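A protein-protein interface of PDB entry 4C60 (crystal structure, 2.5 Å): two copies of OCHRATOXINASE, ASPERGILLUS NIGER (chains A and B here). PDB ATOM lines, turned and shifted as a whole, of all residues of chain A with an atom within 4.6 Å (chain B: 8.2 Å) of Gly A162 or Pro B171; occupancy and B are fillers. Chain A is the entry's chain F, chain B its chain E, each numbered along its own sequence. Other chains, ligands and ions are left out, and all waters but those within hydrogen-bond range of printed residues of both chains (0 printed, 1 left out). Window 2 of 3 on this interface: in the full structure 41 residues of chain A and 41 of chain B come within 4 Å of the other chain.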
ATOM      1  N   GLY A 158      14.104   5.432  19.810  1.00  0.00           N
ATOM      2  CA  GLY A 158      13.007   5.255  20.771  1.00  0.00           C
ATOM      3  C   GLY A 158      11.780   4.563  20.186  1.00  0.00           C
ATOM      4  O   GLY A 158      11.123   3.763  20.859  1.00  0.00           O
ATOM      5  N   GLU A 159      11.499   4.834  18.917  1.00  0.00           N
ATOM      6  CA  GLU A 159      10.457   4.127  18.195  1.00  0.00           C
ATOM      7  C   GLU A 159      10.787   2.641  18.033  1.00  0.00           C
ATOM      8  O   GLU A 159       9.928   1.787  18.274  1.00  0.00           O
ATOM      9  CB  GLU A 159      10.221   4.748  16.812  1.00  0.00           C
ATOM     10  CG  GLU A 159       9.466   6.068  16.820  1.00  0.00           C
ATOM     11  CD  GLU A 159      10.278   7.261  17.288  1.00  0.00           C
ATOM     12  OE1 GLU A 159      11.496   7.130  17.519  1.00  0.00           O
ATOM     13  OE2 GLU A 159       9.684   8.354  17.432  1.00  0.00           O
ATOM     14  N   VAL A 160      12.015   2.321  17.639  1.00  0.00           N
ATOM     15  CA  VAL A 160      12.398   0.914  17.456  1.00  0.00           C
ATOM     16  C   VAL A 160      12.430   0.130  18.769  1.00  0.00           C
ATOM     17  O   VAL A 160      11.884  -0.965  18.843  1.00  0.00           O
ATOM     18  CB  VAL A 160      13.743   0.740  16.714  1.00  0.00           C
ATOM     19  CG1 VAL A 160      14.085  -0.740  16.537  1.00  0.00           C
ATOM     20  CG2 VAL A 160      13.655   1.413  15.350  1.00  0.00           C
ATOM     21  N   LEU A 161      13.043   0.677  19.807  1.00  0.00           N
ATOM     22  CA  LEU A 161      13.113  -0.054  21.069  1.00  0.00           C
ATOM     23  C   LEU A 161      11.780  -0.048  21.835  1.00  0.00           C
ATOM     24  O   LEU A 161      11.532  -0.924  22.675  1.00  0.00           O
ATOM     25  CB  LEU A 161      14.238   0.461  21.969  1.00  0.00           C
ATOM     26  CG  LEU A 161      15.592  -0.207  21.768  1.00  0.00           C
ATOM     27  CD1 LEU A 161      16.329   0.366  20.564  1.00  0.00           C
ATOM     28  CD2 LEU A 161      16.436   0.001  23.009  1.00  0.00           C
ATOM     29  N   GLY A 162      10.936   0.938  21.563  1.00  0.00           N
ATOM     30  CA  GLY A 162       9.581   0.931  22.110  1.00  0.00           C
ATOM     31  C   GLY A 162       8.803  -0.233  21.529  1.00  0.00           C
ATOM     32  O   GLY A 162       8.066  -0.895  22.242  1.00  0.00           O
ATOM     33  N   SER A 163       9.003  -0.492  20.235  1.00  0.00           N
ATOM     34  CA  SER A 163       8.363  -1.621  19.568  1.00  0.00           C
ATOM     35  C   SER A 163       8.973  -2.970  19.908  1.00  0.00           C
ATOM     36  O   SER A 163       8.253  -3.908  20.222  1.00  0.00           O
ATOM     37  CB  SER A 163       8.401  -1.451  18.061  1.00  0.00           C
ATOM     38  OG  SER A 163       7.549  -0.404  17.658  1.00  0.00           O
ATOM     39  N   TYR A 164      10.293  -3.066  19.909  1.00  0.00           N
ATOM     40  CA  TYR A 164      10.945  -4.373  19.963  1.00  0.00           C
ATOM     41  C   TYR A 164      11.861  -4.652  21.166  1.00  0.00           C
ATOM     42  O   TYR A 164      12.396  -5.763  21.283  1.00  0.00           O
ATOM     43  CB  TYR A 164      11.742  -4.550  18.700  1.00  0.00           C
ATOM     44  CG  TYR A 164      10.905  -4.485  17.460  1.00  0.00           C
ATOM     45  CD1 TYR A 164       9.718  -5.186  17.366  1.00  0.00           C
ATOM     46  CD2 TYR A 164      11.311  -3.742  16.363  1.00  0.00           C
ATOM     47  CE1 TYR A 164       8.946  -5.146  16.214  1.00  0.00           C
ATOM     48  CE2 TYR A 164      10.534  -3.680  15.213  1.00  0.00           C
ATOM     49  CZ  TYR A 164       9.356  -4.394  15.143  1.00  0.00           C
ATOM     50  OH  TYR A 164       8.594  -4.365  13.999  1.00  0.00           O
ATOM     51  N   ARG A 170       3.823  -3.417  28.219  1.00  0.00           N
ATOM     52  CA  ARG A 170       2.717  -2.551  27.864  1.00  0.00           C
ATOM     53  C   ARG A 170       1.678  -3.347  27.089  1.00  0.00           C
ATOM     54  O   ARG A 170       1.967  -4.423  26.599  1.00  0.00           O
ATOM     55  CB  ARG A 170       3.225  -1.405  26.988  1.00  0.00           C
ATOM     56  CG  ARG A 170       4.172  -1.871  25.886  1.00  0.00           C
ATOM     57  CD  ARG A 170       4.196  -0.938  24.667  1.00  0.00           C
ATOM     58  NE  ARG A 170       5.114  -1.442  23.651  1.00  0.00           N
ATOM     59  CZ  ARG A 170       4.825  -2.349  22.729  1.00  0.00           C
ATOM     60  NH1 ARG A 170       3.611  -2.857  22.611  1.00  0.00           N
ATOM     61  NH2 ARG A 170       5.770  -2.750  21.897  1.00  0.00           N
ATOM     62  N   PRO A 171       0.462  -2.802  26.956  1.00  0.00           N
ATOM     63  CA  PRO A 171      -0.445  -3.423  26.013  1.00  0.00           C
ATOM     64  C   PRO A 171       0.134  -3.373  24.581  1.00  0.00           C
ATOM     65  O   PRO A 171       1.147  -2.703  24.336  1.00  0.00           O
ATOM     66  CB  PRO A 171      -1.703  -2.556  26.106  1.00  0.00           C
ATOM     67  CG  PRO A 171      -1.616  -1.891  27.444  1.00  0.00           C
ATOM     68  CD  PRO A 171      -0.158  -1.681  27.681  1.00  0.00           C
ATOM     69  N   GLY B 162      -6.065   0.080  28.395  1.00  0.00           N
ATOM     70  CA  GLY B 162      -4.693   0.143  27.931  1.00  0.00           C
ATOM     71  C   GLY B 162      -4.645  -0.406  26.520  1.00  0.00           C
ATOM     72  O   GLY B 162      -3.941   0.136  25.675  1.00  0.00           O
ATOM     73  N   ASN B 168      -3.149   7.757  25.746  1.00  0.00           N
ATOM     74  CA  ASN B 168      -1.854   7.080  25.882  1.00  0.00           C
ATOM     75  C   ASN B 168      -1.382   6.370  24.634  1.00  0.00           C
ATOM     76  O   ASN B 168      -1.233   5.149  24.623  1.00  0.00           O
ATOM     77  CB  ASN B 168      -1.882   6.106  27.057  1.00  0.00           C
ATOM     78  CG  ASN B 168      -2.065   6.820  28.359  1.00  0.00           C
ATOM     79  OD1 ASN B 168      -3.135   6.779  28.978  1.00  0.00           O
ATOM     80  ND2 ASN B 168      -1.033   7.517  28.766  1.00  0.00           N
ATOM     81  N   PRO B 169      -1.106   7.140  23.583  1.00  0.00           N
ATOM     82  CA  PRO B 169      -0.473   6.524  22.425  1.00  0.00           C
ATOM     83  C   PRO B 169       0.864   5.870  22.779  1.00  0.00           C
ATOM     84  O   PRO B 169       1.562   6.323  23.661  1.00  0.00           O
ATOM     85  CB  PRO B 169      -0.283   7.698  21.470  1.00  0.00           C
ATOM     86  CG  PRO B 169      -0.354   8.919  22.327  1.00  0.00           C
ATOM     87  CD  PRO B 169      -1.334   8.576  23.392  1.00  0.00           C
ATOM     88  N   ARG B 170       1.169   4.772  22.104  1.00  0.00           N
ATOM     89  CA  ARG B 170       2.269   3.903  22.468  1.00  0.00           C
ATOM     90  C   ARG B 170       2.579   2.982  21.319  1.00  0.00           C
ATOM     91  O   ARG B 170       1.798   2.847  20.382  1.00  0.00           O
ATOM     92  CB  ARG B 170       1.877   3.040  23.660  1.00  0.00           C
ATOM     93  CG  ARG B 170       0.479   2.425  23.526  1.00  0.00           C
ATOM     94  CD  ARG B 170       0.299   1.133  24.304  1.00  0.00           C
ATOM     95  NE  ARG B 170      -1.046   0.617  24.103  1.00  0.00           N
ATOM     96  CZ  ARG B 170      -1.445  -0.177  23.109  1.00  0.00           C
ATOM     97  NH1 ARG B 170      -0.597  -0.593  22.181  1.00  0.00           N
ATOM     98  NH2 ARG B 170      -2.722  -0.562  23.041  1.00  0.00           N
ATOM     99  N   PRO B 171       3.752   2.341  21.366  1.00  0.00           N
ATOM    100  CA  PRO B 171       3.986   1.305  20.359  1.00  0.00           C
ATOM    101  C   PRO B 171       2.977   0.176  20.509  1.00  0.00           C
ATOM    102  O   PRO B 171       2.226   0.150  21.502  1.00  0.00           O
ATOM    103  CB  PRO B 171       5.407   0.809  20.674  1.00  0.00           C
ATOM    104  CG  PRO B 171       6.047   1.942  21.388  1.00  0.00           C
ATOM    105  CD  PRO B 171       4.954   2.619  22.169  1.00  0.00           C
ATOM    106  N   GLY B 172       2.947  -0.715  19.517  1.00  0.00           N
ATOM    107  CA  GLY B 172       2.104  -1.918  19.563  1.00  0.00           C
ATOM    108  C   GLY B 172       0.751  -1.797  18.882  1.00  0.00           C
ATOM    109  O   GLY B 172      -0.252  -2.250  19.408  1.00  0.00           O
ATOM    110  N   TYR B 173       0.723  -1.155  17.720  1.00  0.00           N
ATOM    111  CA  TYR B 173      -0.495  -1.062  16.907  1.00  0.00           C
ATOM    112  C   TYR B 173      -1.667  -0.472  17.679  1.00  0.00           C
ATOM    113  O   TYR B 173      -2.800  -0.938  17.573  1.00  0.00           O
ATOM    114  CB  TYR B 173      -0.815  -2.438  16.311  1.00  0.00           C
ATOM    115  CG  TYR B 173       0.371  -2.999  15.535  1.00  0.00           C
ATOM    116  CD1 TYR B 173       0.762  -2.426  14.327  1.00  0.00           C
ATOM    117  CD2 TYR B 173       1.134  -4.072  16.025  1.00  0.00           C
ATOM    118  CE1 TYR B 173       1.850  -2.919  13.606  1.00  0.00           C
ATOM    119  CE2 TYR B 173       2.230  -4.564  15.309  1.00  0.00           C
ATOM    120  CZ  TYR B 173       2.580  -3.985  14.091  1.00  0.00           C
ATOM    121  OH  TYR B 173       3.628  -4.451  13.346  1.00  0.00           O
ATOM    122  N   TRP B 174      -1.369   0.560  18.464  1.00  0.00           N
ATOM    123  CA  TRP B 174      -2.368   1.315  19.218  1.00  0.00           C
ATOM    124  C   TRP B 174      -3.457   1.825  18.279  1.00  0.00           C
ATOM    125  O   TRP B 174      -3.162   2.234  17.155  1.00  0.00           O
ATOM    126  CB  TRP B 174      -1.669   2.483  19.893  1.00  0.00           C
ATOM    127  CG  TRP B 174      -2.510   3.385  20.766  1.00  0.00           C
ATOM    128  CD1 TRP B 174      -2.863   3.172  22.060  1.00  0.00           C
ATOM    129  CD2 TRP B 174      -3.019   4.691  20.415  1.00  0.00           C
ATOM    130  NE1 TRP B 174      -3.578   4.241  22.524  1.00  0.00           N
ATOM    131  CE2 TRP B 174      -3.689   5.186  21.536  1.00  0.00           C
ATOM    132  CE3 TRP B 174      -2.968   5.475  19.255  1.00  0.00           C
ATOM    133  CZ2 TRP B 174      -4.309   6.424  21.548  1.00  0.00           C
ATOM    134  CZ3 TRP B 174      -3.610   6.691  19.252  1.00  0.00           C
ATOM    135  CH2 TRP B 174      -4.273   7.159  20.397  1.00  0.00           C
ATOM    136  N   GLY B 175      -4.710   1.770  18.737  1.00  0.00           N
ATOM    137  CA  GLY B 175      -5.847   2.230  17.968  1.00  0.00           C
ATOM    138  C   GLY B 175      -6.237   1.347  16.808  1.00  0.00           C
ATOM    139  O   GLY B 175      -6.924   1.806  15.887  1.00  0.00           O
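NH1 of Arg B170 is in hydrogen-bond range of O of Pro A171, 3.5 Å away.
The guanidinium group (NH1) of Arg A170 lies within hydrogen-bond range of the backbone carbonyl oxygen (O) of Pro B171, at 3.5 Å.
Among the printed residues, merely in contact across the chains: Gly A162 with Pro B171 (3.5 Å), Ser A163 with Pro B171 (3.8 Å), Arg A170 with Gly B172 (3.5 Å) and Pro A171 with Gly B162 (3.5 Å).
NH2 of Arg B170 sits at hydrogen-bond distance from O of Gly B162 (3.0 Å).
The guanidinium group of Arg B170 sits at hydrogen-bond distance from the backbone carbonyl oxygen of Gly B172.
OG of Ser A163 is in hydrogen-bond range of O of Glu A159 (3.3 Å).
The guanidinium group (NH2) of Arg A170 lies within hydrogen-bond range of the backbone carbonyl oxygen (O) of Ser A163 (3.2 Å).
NH2 of Arg A170 is in hydrogen-bond range of O of Gly A162.
Gly A162 touches Pro B171, and with the chains exchanged Pro A171 touches Gly B162.
Arg A170 touches Pro B171, and with the chains exchanged Pro A171 touches Arg B170.
Of the 6 pairs that touch across the chains among the printed residues, 4 have their exchanged pair printed and touching as well.
Of the 9 printed residues of chain A, 4 touch a printed residue of chain B.
Hydrophobic or aromatic side chains of chain A within 4 Å of the printed part of chain B: Pro A171.
Of the 9 printed residues of chain B, 4 touch a printed residue of chain A.
Among the printed residues, no Asp or Glu carboxylate lies within 4 Å of a Lys or Arg side-chain nitrogen of the other chain.
Gly A158 touches none of the printed residues of chain B.
Of chain B, only Pro B171 (3.5 Å) comes within 4 Å of Gly A162.
Of the printed residues of chain B, Ser A163 touches Pro B171 (3.8 Å).
Tyr A164 touches none of the printed residues of chain B.
Of the printed residues of chain B, Arg A170 touches Pro B171 (3.5 Å) and Gly B172 (3.5 Å).
Of the printed residues of chain B, Pro A171 touches Gly B162 and Arg B170.
Of the printed residues of chain A, Gly B162 touches Pro A171 (3.5 Å).
Printed residues of chain A within 4 Å of Arg B170: Pro A171.
Of chain A, only Gly A162, Ser A163 and Arg A170 come within 4 Å of Pro B171.
Of the printed residues of chain A, Gly B172 touches Arg A170 (3.5 Å).
The nearest residue of chain B that does not touch Gly A162 is Gly B172 (5.8 Å).
The nearest residue of chain A that does not touch Pro B171 is Pro A171 (4.2 Å).
The nearest printed residue of chain A that does not touch Gly B172 is Pro A171 (4.9 Å).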
